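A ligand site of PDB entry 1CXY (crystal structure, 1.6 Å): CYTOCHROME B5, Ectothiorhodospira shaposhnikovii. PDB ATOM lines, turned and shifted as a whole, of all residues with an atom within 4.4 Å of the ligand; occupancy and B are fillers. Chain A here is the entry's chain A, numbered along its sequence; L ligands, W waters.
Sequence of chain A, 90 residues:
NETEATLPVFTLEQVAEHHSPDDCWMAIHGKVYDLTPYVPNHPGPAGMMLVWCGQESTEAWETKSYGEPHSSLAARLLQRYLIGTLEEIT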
ATOM      1  N   MET A  26     -19.986 -12.468 -26.605  1.00  0.00           N
ATOM      2  CA  MET A  26     -19.685 -12.752 -25.199  1.00  0.00           C
ATOM      3  C   MET A  26     -20.646 -13.811 -24.663  1.00  0.00           C
ATOM      4  O   MET A  26     -21.705 -13.953 -25.232  1.00  0.00           O
ATOM      5  CB  MET A  26     -19.890 -11.556 -24.263  1.00  0.00           C
ATOM      6  CG  MET A  26     -18.953 -10.415 -24.572  1.00  0.00           C
ATOM      7  SD  MET A  26     -19.208  -9.079 -23.392  1.00  0.00           S
ATOM      8  CE  MET A  26     -18.192  -7.861 -24.239  1.00  0.00           C
ATOM      9  N   LEU A  35     -22.336  -9.006 -29.867  1.00  0.00           N
ATOM     10  CA  LEU A  35     -22.360  -7.593 -29.501  1.00  0.00           C
ATOM     11  C   LEU A  35     -21.606  -6.658 -30.414  1.00  0.00           C
ATOM     12  O   LEU A  35     -21.480  -5.442 -30.168  1.00  0.00           O
ATOM     13  CB  LEU A  35     -21.803  -7.532 -28.063  1.00  0.00           C
ATOM     14  CG  LEU A  35     -22.778  -8.098 -27.010  1.00  0.00           C
ATOM     15  CD1 LEU A  35     -22.069  -8.517 -25.726  1.00  0.00           C
ATOM     16  CD2 LEU A  35     -23.860  -7.061 -26.695  1.00  0.00           C
ATOM     17  N   TYR A  38     -23.153  -3.377 -31.157  1.00  0.00           N
ATOM     18  CA  TYR A  38     -23.312  -2.528 -29.960  1.00  0.00           C
ATOM     19  C   TYR A  38     -22.031  -1.859 -29.518  1.00  0.00           C
ATOM     20  O   TYR A  38     -22.076  -0.766 -28.940  1.00  0.00           O
ATOM     21  CB  TYR A  38     -23.912  -3.372 -28.826  1.00  0.00           C
ATOM     22  CG  TYR A  38     -24.172  -2.507 -27.608  1.00  0.00           C
ATOM     23  CD1 TYR A  38     -23.293  -2.521 -26.534  1.00  0.00           C
ATOM     24  CD2 TYR A  38     -25.222  -1.591 -27.626  1.00  0.00           C
ATOM     25  CE1 TYR A  38     -23.500  -1.662 -25.464  1.00  0.00           C
ATOM     26  CE2 TYR A  38     -25.428  -0.741 -26.552  1.00  0.00           C
ATOM     27  CZ  TYR A  38     -24.564  -0.772 -25.488  1.00  0.00           C
ATOM     28  OH  TYR A  38     -24.767   0.091 -24.438  1.00  0.00           O
ATOM     29  N   HIS A  42     -21.483   1.611 -26.529  1.00  0.00           N
ATOM     30  CA  HIS A  42     -21.415   1.399 -25.081  1.00  0.00           C
ATOM     31  C   HIS A  42     -21.032   2.688 -24.350  1.00  0.00           C
ATOM     32  O   HIS A  42     -20.018   3.289 -24.694  1.00  0.00           O
ATOM     33  CB  HIS A  42     -20.368   0.316 -24.789  1.00  0.00           C
ATOM     34  CG  HIS A  42     -20.303  -0.080 -23.346  1.00  0.00           C
ATOM     35  ND1 HIS A  42     -19.181  -0.011 -22.560  1.00  0.00           N
ATOM     36  CD2 HIS A  42     -21.313  -0.519 -22.543  1.00  0.00           C
ATOM     37  CE1 HIS A  42     -19.462  -0.417 -21.342  1.00  0.00           C
ATOM     38  NE2 HIS A  42     -20.744  -0.722 -21.296  1.00  0.00           N
ATOM     39  N   PRO A  43     -21.805   3.082 -23.358  1.00  0.00           N
ATOM     40  CA  PRO A  43     -21.512   4.280 -22.556  1.00  0.00           C
ATOM     41  C   PRO A  43     -20.301   4.040 -21.650  1.00  0.00           C
ATOM     42  O   PRO A  43     -19.777   2.929 -21.518  1.00  0.00           O
ATOM     43  CB  PRO A  43     -22.756   4.491 -21.722  1.00  0.00           C
ATOM     44  CG  PRO A  43     -23.814   3.640 -22.345  1.00  0.00           C
ATOM     45  CD  PRO A  43     -23.040   2.429 -22.852  1.00  0.00           C
ATOM     46  N   GLY A  44     -19.810   5.096 -21.006  1.00  0.00           N
ATOM     47  CA  GLY A  44     -18.688   4.977 -20.090  1.00  0.00           C
ATOM     48  C   GLY A  44     -17.332   5.141 -20.736  1.00  0.00           C
ATOM     49  O   GLY A  44     -17.164   5.450 -21.919  1.00  0.00           O
ATOM     50  N   PRO A  45     -16.293   4.862 -19.964  1.00  0.00           N
ATOM     51  CA  PRO A  45     -14.908   4.986 -20.412  1.00  0.00           C
ATOM     52  C   PRO A  45     -14.670   4.160 -21.660  1.00  0.00           C
ATOM     53  O   PRO A  45     -15.112   3.020 -21.770  1.00  0.00           O
ATOM     54  CB  PRO A  45     -14.077   4.525 -19.222  1.00  0.00           C
ATOM     55  CG  PRO A  45     -14.965   4.833 -18.047  1.00  0.00           C
ATOM     56  CD  PRO A  45     -16.349   4.457 -18.530  1.00  0.00           C
ATOM     57  N   MET A  48     -14.047  -0.342 -22.404  1.00  0.00           N
ATOM     58  CA  MET A  48     -14.180  -1.263 -21.287  1.00  0.00           C
ATOM     59  C   MET A  48     -14.791  -2.606 -21.627  1.00  0.00           C
ATOM     60  O   MET A  48     -14.566  -3.666 -21.029  1.00  0.00           O
ATOM     61  CB  MET A  48     -15.126  -0.566 -20.261  1.00  0.00           C
ATOM     62  CG  MET A  48     -14.291   0.550 -19.627  1.00  0.00           C
ATOM     63  SD  MET A  48     -13.379  -0.187 -18.255  1.00  0.00           S
ATOM     64  CE  MET A  48     -14.702  -0.806 -17.228  1.00  0.00           C
ATOM     65  N   MET A  49     -15.672  -2.563 -22.624  1.00  0.00           N
ATOM     66  CA  MET A  49     -16.329  -3.819 -23.029  1.00  0.00           C
ATOM     67  C   MET A  49     -15.413  -4.640 -23.890  1.00  0.00           C
ATOM     68  O   MET A  49     -15.415  -5.878 -23.864  1.00  0.00           O
ATOM     69  CB  MET A  49     -17.620  -3.330 -23.702  1.00  0.00           C
ATOM     70  CG  MET A  49     -18.676  -4.393 -23.892  1.00  0.00           C
ATOM     71  SD  MET A  49     -20.021  -3.644 -24.855  1.00  0.00           S
ATOM     72  CE  MET A  49     -20.782  -5.126 -25.486  1.00  0.00           C
ATOM     73  N   TRP A  52     -13.599  -7.919 -22.886  1.00  0.00           N
ATOM     74  CA  TRP A  52     -14.400  -9.126 -22.714  1.00  0.00           C
ATOM     75  C   TRP A  52     -14.868  -9.751 -24.023  1.00  0.00           C
ATOM     76  O   TRP A  52     -15.476 -10.832 -23.948  1.00  0.00           O
ATOM     77  CB  TRP A  52     -15.627  -8.828 -21.796  1.00  0.00           C
ATOM     78  CG  TRP A  52     -15.079  -8.358 -20.467  1.00  0.00           C
ATOM     79  CD1 TRP A  52     -14.925  -7.092 -20.011  1.00  0.00           C
ATOM     80  CD2 TRP A  52     -14.455  -9.228 -19.524  1.00  0.00           C
ATOM     81  NE1 TRP A  52     -14.250  -7.106 -18.809  1.00  0.00           N
ATOM     82  CE2 TRP A  52     -13.949  -8.407 -18.479  1.00  0.00           C
ATOM     83  CE3 TRP A  52     -14.284 -10.613 -19.432  1.00  0.00           C
ATOM     84  CZ2 TRP A  52     -13.302  -8.946 -17.380  1.00  0.00           C
ATOM     85  CZ3 TRP A  52     -13.634 -11.155 -18.342  1.00  0.00           C
ATOM     86  CH2 TRP A  52     -13.150 -10.304 -17.324  1.00  0.00           C
ATOM     87  N   SER A  57     -18.157 -13.499 -19.472  1.00  0.00           N
ATOM     88  CA  SER A  57     -18.017 -12.174 -18.909  1.00  0.00           C
ATOM     89  C   SER A  57     -19.066 -11.831 -17.846  1.00  0.00           C
ATOM     90  O   SER A  57     -19.325 -10.650 -17.621  1.00  0.00           O
ATOM     91  CB  SER A  57     -18.174 -11.167 -20.072  1.00  0.00           C
ATOM     92  OG  SER A  57     -17.267 -11.477 -21.142  1.00  0.00           O
ATOM     93  N   ALA A  60     -17.925  -9.254 -14.966  1.00  0.00           N
ATOM     94  CA  ALA A  60     -17.808  -7.892 -15.504  1.00  0.00           C
ATOM     95  C   ALA A  60     -19.190  -7.321 -15.783  1.00  0.00           C
ATOM     96  O   ALA A  60     -19.403  -6.136 -15.535  1.00  0.00           O
ATOM     97  CB  ALA A  60     -16.975  -7.941 -16.772  1.00  0.00           C
ATOM     98  N   TRP A  61     -20.112  -8.111 -16.323  1.00  0.00           N
ATOM     99  CA  TRP A  61     -21.477  -7.634 -16.543  1.00  0.00           C
ATOM    100  C   TRP A  61     -22.150  -7.239 -15.238  1.00  0.00           C
ATOM    101  O   TRP A  61     -22.920  -6.271 -15.151  1.00  0.00           O
ATOM    102  CB  TRP A  61     -22.293  -8.710 -17.305  1.00  0.00           C
ATOM    103  CG  TRP A  61     -23.766  -8.399 -17.303  1.00  0.00           C
ATOM    104  CD1 TRP A  61     -24.698  -9.023 -16.535  1.00  0.00           C
ATOM    105  CD2 TRP A  61     -24.460  -7.389 -18.050  1.00  0.00           C
ATOM    106  NE1 TRP A  61     -25.932  -8.454 -16.728  1.00  0.00           N
ATOM    107  CE2 TRP A  61     -25.819  -7.469 -17.665  1.00  0.00           C
ATOM    108  CE3 TRP A  61     -24.090  -6.458 -19.016  1.00  0.00           C
ATOM    109  CZ2 TRP A  61     -26.783  -6.623 -18.214  1.00  0.00           C
ATOM    110  CZ3 TRP A  61     -25.055  -5.618 -19.553  1.00  0.00           C
ATOM    111  CH2 TRP A  61     -26.386  -5.707 -19.145  1.00  0.00           C
ATOM    112  N   LYS A  64     -19.601  -4.197 -13.538  1.00  0.00           N
ATOM    113  CA  LYS A  64     -18.960  -3.173 -14.349  1.00  0.00           C
ATOM    114  C   LYS A  64     -17.466  -3.071 -13.972  1.00  0.00           C
ATOM    115  O   LYS A  64     -16.798  -2.066 -14.212  1.00  0.00           O
ATOM    116  CB  LYS A  64     -19.637  -1.812 -14.249  1.00  0.00           C
ATOM    117  CG  LYS A  64     -21.027  -1.786 -14.892  1.00  0.00           C
ATOM    118  CD  LYS A  64     -21.732  -0.461 -14.623  1.00  0.00           C
ATOM    119  CE  LYS A  64     -23.061  -0.445 -15.398  1.00  0.00           C
ATOM    120  NZ  LYS A  64     -23.994   0.604 -14.870  1.00  0.00           N
ATOM    121  N   SER A  65     -16.929  -4.089 -13.311  1.00  0.00           N
ATOM    122  CA  SER A  65     -15.575  -4.186 -12.818  1.00  0.00           C
ATOM    123  C   SER A  65     -15.245  -3.190 -11.706  1.00  0.00           C
ATOM    124  O   SER A  65     -14.078  -3.211 -11.292  1.00  0.00           O
ATOM    125  CB  SER A  65     -14.533  -4.072 -13.950  1.00  0.00           C
ATOM    126  OG  SER A  65     -14.608  -5.302 -14.712  1.00  0.00           O
ATOM    127  N   TYR A  66     -16.184  -2.476 -11.122  1.00  0.00           N
ATOM    128  CA  TYR A  66     -15.853  -1.611  -9.987  1.00  0.00           C
ATOM    129  C   TYR A  66     -16.931  -1.696  -8.908  1.00  0.00           C
ATOM    130  O   TYR A  66     -16.697  -1.181  -7.814  1.00  0.00           O
ATOM    131  CB  TYR A  66     -15.634  -0.181 -10.433  1.00  0.00           C
ATOM    132  CG  TYR A  66     -16.846   0.654 -10.786  1.00  0.00           C
ATOM    133  CD1 TYR A  66     -17.275   1.676  -9.953  1.00  0.00           C
ATOM    134  CD2 TYR A  66     -17.537   0.432 -11.978  1.00  0.00           C
ATOM    135  CE1 TYR A  66     -18.356   2.459 -10.285  1.00  0.00           C
ATOM    136  CE2 TYR A  66     -18.616   1.222 -12.322  1.00  0.00           C
ATOM    137  CZ  TYR A  66     -19.035   2.221 -11.468  1.00  0.00           C
ATOM    138  OH  TYR A  66     -20.088   3.049 -11.774  1.00  0.00           O
ATOM    139  N   GLU A  68     -20.823  -1.679  -9.600  1.00  0.00           N
ATOM    140  CA  GLU A  68     -22.167  -1.145  -9.878  1.00  0.00           C
ATOM    141  C   GLU A  68     -22.797  -2.083 -10.908  1.00  0.00           C
ATOM    142  O   GLU A  68     -22.115  -2.447 -11.848  1.00  0.00           O
ATOM    143  CB  GLU A  68     -22.109   0.254 -10.468  1.00  0.00           C
ATOM    144  N   PRO A  69     -24.045  -2.470 -10.747  1.00  0.00           N
ATOM    145  CA  PRO A  69     -24.682  -3.326 -11.730  1.00  0.00           C
ATOM    146  C   PRO A  69     -25.084  -2.535 -12.954  1.00  0.00           C
ATOM    147  O   PRO A  69     -25.200  -1.308 -12.999  1.00  0.00           O
ATOM    148  CB  PRO A  69     -25.958  -3.777 -10.987  1.00  0.00           C
ATOM    149  CG  PRO A  69     -26.288  -2.596 -10.136  1.00  0.00           C
ATOM    150  CD  PRO A  69     -24.955  -2.076  -9.651  1.00  0.00           C
ATOM    151  N   HIS A  70     -25.358  -3.267 -14.041  1.00  0.00           N
ATOM    152  CA  HIS A  70     -26.023  -2.658 -15.179  1.00  0.00           C
ATOM    153  C   HIS A  70     -27.514  -2.495 -14.847  1.00  0.00           C
ATOM    154  O   HIS A  70     -28.120  -3.290 -14.126  1.00  0.00           O
ATOM    155  CB  HIS A  70     -25.892  -3.472 -16.473  1.00  0.00           C
ATOM    156  CG  HIS A  70     -24.552  -3.242 -17.112  1.00  0.00           C
ATOM    157  ND1 HIS A  70     -23.474  -4.043 -16.797  1.00  0.00           N
ATOM    158  CD2 HIS A  70     -24.140  -2.326 -18.017  1.00  0.00           C
ATOM    159  CE1 HIS A  70     -22.419  -3.634 -17.490  1.00  0.00           C
ATOM    160  NE2 HIS A  70     -22.791  -2.610 -18.249  1.00  0.00           N
ATOM    161  N   SER A  71     -28.030  -1.397 -15.389  1.00  0.00           N
ATOM    162  CA  SER A  71     -29.451  -1.100 -15.126  1.00  0.00           C
ATOM    163  C   SER A  71     -30.360  -2.098 -15.821  1.00  0.00           C
ATOM    164  O   SER A  71     -29.954  -2.883 -16.675  1.00  0.00           O
ATOM    165  CB  SER A  71     -29.753   0.302 -15.644  1.00  0.00           C
ATOM    166  OG  SER A  71     -29.757   0.319 -17.061  1.00  0.00           O
ATOM    167  N   LEU A  73     -32.602  -1.088 -17.914  1.00  0.00           N
ATOM    168  CA  LEU A  73     -32.530  -0.626 -19.286  1.00  0.00           C
ATOM    169  C   LEU A  73     -31.393  -1.346 -20.010  1.00  0.00           C
ATOM    170  O   LEU A  73     -31.553  -1.857 -21.117  1.00  0.00           O
ATOM    171  CB  LEU A  73     -32.364   0.890 -19.371  1.00  0.00           C
ATOM    172  CG  LEU A  73     -32.124   1.541 -20.727  1.00  0.00           C
ATOM    173  CD1 LEU A  73     -32.408   3.049 -20.652  1.00  0.00           C
ATOM    174  CD2 LEU A  73     -30.679   1.385 -21.194  1.00  0.00           C
ATOM    175  N   ALA A  74     -30.199  -1.344 -19.399  1.00  0.00           N
ATOM    176  CA  ALA A  74     -29.060  -2.043 -20.009  1.00  0.00           C
ATOM    177  C   ALA A  74     -29.332  -3.524 -20.195  1.00  0.00           C
ATOM    178  O   ALA A  74     -28.885  -4.086 -21.212  1.00  0.00           O
ATOM    179  CB  ALA A  74     -27.805  -1.826 -19.159  1.00  0.00           C
ATOM    180  N   LEU A  77     -31.329  -3.974 -23.254  1.00  0.00           N
ATOM    181  CA  LEU A  77     -30.495  -3.764 -24.434  1.00  0.00           C
ATOM    182  C   LEU A  77     -29.609  -4.981 -24.677  1.00  0.00           C
ATOM    183  O   LEU A  77     -29.474  -5.407 -25.829  1.00  0.00           O
ATOM    184  CB  LEU A  77     -29.622  -2.526 -24.290  1.00  0.00           C
ATOM    185  CG  LEU A  77     -30.295  -1.152 -24.215  1.00  0.00           C
ATOM    186  CD1 LEU A  77     -29.200  -0.104 -24.053  1.00  0.00           C
ATOM    187  CD2 LEU A  77     -31.107  -0.874 -25.468  1.00  0.00           C
ATOM    188  N   LEU A  78     -29.040  -5.593 -23.631  1.00  0.00           N
ATOM    189  CA  LEU A  78     -28.207  -6.778 -23.801  1.00  0.00           C
ATOM    190  C   LEU A  78     -29.002  -7.910 -24.462  1.00  0.00           C
ATOM    191  O   LEU A  78     -28.530  -8.541 -25.383  1.00  0.00           O
ATOM    192  CB  LEU A  78     -27.642  -7.268 -22.458  1.00  0.00           C
ATOM    193  CG  LEU A  78     -26.970  -8.659 -22.463  1.00  0.00           C
ATOM    194  CD1 LEU A  78     -25.745  -8.675 -23.401  1.00  0.00           C
ATOM    195  CD2 LEU A  78     -26.530  -9.095 -21.075  1.00  0.00           C
ATOM    196  N   TYR A  81     -29.234  -8.569 -28.262  1.00  0.00           N
ATOM    197  CA  TYR A  81     -28.102  -9.131 -29.019  1.00  0.00           C
ATOM    198  C   TYR A  81     -27.944 -10.612 -28.778  1.00  0.00           C
ATOM    199  O   TYR A  81     -26.978 -11.232 -29.234  1.00  0.00           O
ATOM    200  CB  TYR A  81     -26.835  -8.349 -28.620  1.00  0.00           C
ATOM    201  CG  TYR A  81     -26.968  -6.889 -29.011  1.00  0.00           C
ATOM    202  CD1 TYR A  81     -27.250  -5.947 -28.011  1.00  0.00           C
ATOM    203  CD2 TYR A  81     -26.891  -6.495 -30.337  1.00  0.00           C
ATOM    204  CE1 TYR A  81     -27.417  -4.623 -28.355  1.00  0.00           C
ATOM    205  CE2 TYR A  81     -27.054  -5.147 -30.676  1.00  0.00           C
ATOM    206  CZ  TYR A  81     -27.337  -4.248 -29.674  1.00  0.00           C
ATOM    207  OH  TYR A  81     -27.524  -2.914 -29.983  1.00  0.00           O
HETATM  208  C1  LIG L   1     -22.422   1.565 -18.567  1.00  0.00           C
HETATM  209  C2  LIG L   1     -18.868  -1.654 -17.955  1.00  0.00           C
HETATM  210  C3  LIG L   1     -21.078  -4.631 -21.058  1.00  0.00           C
HETATM  211  C4  LIG L   1     -24.705  -1.462 -21.575  1.00  0.00           C
HETATM  212  C5  LIG L   1     -21.223   1.005 -18.224  1.00  0.00           C
HETATM  213  C6  LIG L   1     -20.146   1.660 -17.496  1.00  0.00           C
HETATM  214  C7  LIG L   1     -19.185   0.744 -17.307  1.00  0.00           C
HETATM  215  C8  LIG L   1     -19.610  -0.492 -17.937  1.00  0.00           C
HETATM  216  C9  LIG L   1     -17.828   0.911 -16.596  1.00  0.00           C
HETATM  217  C10 LIG L   1     -20.169   3.119 -16.981  1.00  0.00           C
HETATM  218  C11 LIG L   1     -20.232   3.276 -15.423  1.00  0.00           C
HETATM  219  C12 LIG L   1     -21.602   3.015 -14.859  1.00  0.00           C
HETATM  220  O1  LIG L   1     -22.587   3.092 -15.645  1.00  0.00           O
HETATM  221  O2  LIG L   1     -21.737   2.757 -13.639  1.00  0.00           O
HETATM  222  C13 LIG L   1     -19.186  -2.764 -18.718  1.00  0.00           C
HETATM  223  C14 LIG L   1     -18.422  -3.991 -18.774  1.00  0.00           C
HETATM  224  C15 LIG L   1     -19.043  -4.822 -19.608  1.00  0.00           C
HETATM  225  C16 LIG L   1     -20.201  -4.130 -20.127  1.00  0.00           C
HETATM  226  C17 LIG L   1     -17.145  -4.233 -17.926  1.00  0.00           C
HETATM  227  C18 LIG L   1     -18.635  -6.268 -19.985  1.00  0.00           C
HETATM  228  C19 LIG L   1     -19.518  -7.250 -20.131  1.00  0.00           C
HETATM  229  C20 LIG L   1     -22.249  -4.030 -21.473  1.00  0.00           C
HETATM  230  C21 LIG L   1     -23.195  -4.588 -22.415  1.00  0.00           C
HETATM  231  C22 LIG L   1     -24.210  -3.722 -22.549  1.00  0.00           C
HETATM  232  C23 LIG L   1     -23.919  -2.587 -21.682  1.00  0.00           C
HETATM  233  C24 LIG L   1     -23.001  -5.971 -23.072  1.00  0.00           C
HETATM  234  C25 LIG L   1     -25.521  -3.814 -23.359  1.00  0.00           C
HETATM  235  C26 LIG L   1     -25.612  -4.283 -24.581  1.00  0.00           C
HETATM  236  C27 LIG L   1     -24.396  -0.384 -20.783  1.00  0.00           C
HETATM  237  C28 LIG L   1     -25.291   0.725 -20.538  1.00  0.00           C
HETATM  238  C29 LIG L   1     -24.660   1.558 -19.702  1.00  0.00           C
HETATM  239  C30 LIG L   1     -23.372   0.998 -19.388  1.00  0.00           C
HETATM  240  C31 LIG L   1     -26.698   0.870 -21.171  1.00  0.00           C
HETATM  241  C32 LIG L   1     -25.191   2.871 -19.063  1.00  0.00           C
HETATM  242  C33 LIG L   1     -25.504   2.586 -17.567  1.00  0.00           C
HETATM  243  C34 LIG L   1     -26.523   1.506 -17.325  1.00  0.00           C
HETATM  244  O3  LIG L   1     -26.302   0.585 -16.501  1.00  0.00           O
HETATM  245  O4  LIG L   1     -27.624   1.567 -17.942  1.00  0.00           O
HETATM  246  N1  LIG L   1     -20.852  -0.302 -18.506  1.00  0.00           N
HETATM  247  N2  LIG L   1     -20.287  -2.874 -19.561  1.00  0.00           N
HETATM  248  N3  LIG L   1     -22.703  -2.796 -21.070  1.00  0.00           N
HETATM  249  N4  LIG L   1     -23.232  -0.212 -20.052  1.00  0.00           N
HETATM  250 FE1  LIG L   1     -21.795  -1.569 -19.764  1.00  0.00          FE
HETATM  251  O   HOH W   1     -24.033   4.856 -12.521  1.00  0.00           O
HETATM  252  O   HOH W   2     -28.725   3.859 -18.605  1.00  0.00           O
HETATM  253  O   HOH W   3     -23.141   5.178 -17.352  1.00  0.00           O
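O3 of the ligand is in salt-bridge range of NZ of Lys 64.
OG of Ser 71 is in hydrogen-bond range of O4 of the ligand, at 2.6 Å.
NE2 of His 42 binds FE1 of the ligand, 2.0 Å away.
An oxygen (O3) of the ligand lies within hydrogen-bond range of the backbone NH (N) of Ser 71.
NE2 of His 70 is bound to FE1 of the ligand (2.1 Å).
The side-chain hydroxyl (OH) of Tyr 66 lies within hydrogen-bond range of an oxygen (O2) of the ligand, 2.5 Å away.
The side-chain hydroxyl (OG) of Ser 71 is in hydrogen-bond range of the backbone NH (N) of Ala 74, 2.9 Å away.
ND1 of His 70 sits at hydrogen-bond distance from O of Trp 61 (2.8 Å).
The backbone carbonyl oxygen of Pro 69 is in hydrogen-bond range of the side-chain amino group of Lys 64 (2.9 Å).
The side-chain hydroxyl of Ser 71 sits close to the backbone NH of Leu 73 (3.3 Å).
O of Trp 52 sits close to OG of Ser 57, at 3.4 Å.
Met 26 touches the ligand (SD to C19, 3.8 Å).
Leu 35 touches the ligand (CD1 to C24, 3.8 Å).
Tyr 38 touches the ligand (OH to C4, 3.3 Å).
Pro 43 touches the ligand (CG to C29, 3.5 Å).
CA of Gly 44 touches C10 of the ligand, 3.9 Å away.
CE of Met 48 touches C9 of the ligand, at 3.6 Å.
Met 49 touches the ligand (CE to C24, 3.4 Å).
CD1 of Trp 52 touches C18 of the ligand, at 3.8 Å.
Ala 60 touches the ligand.
Trp 61 touches the ligand (CZ3 to C21, 3.6 Å).
Ala 74 touches the ligand (CB to C31, 3.5 Å).
CD1 of Leu 77 touches C31 of the ligand (3.9 Å).
CA of Leu 78 touches C26 of the ligand (3.7 Å).
Hydrophobic or aromatic side chains within 4 Å of the ligand: Met 26, Leu 35, Tyr 38, His 42, Pro 43, Met 48, Met 49, Trp 52, Ala 60, Trp 61, Tyr 66, His 70, Ala 74, Leu 77 and Leu 78.
18 residues have an atom within 4 Å of the ligand: Met 26, Leu 35, Tyr 38, His 42, Pro 43, Gly 44, Met 48, Met 49, Trp 52, Ala 60, Trp 61, Lys 64, Tyr 66, His 70, Ser 71, Ala 74, Leu 77 and Leu 78.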
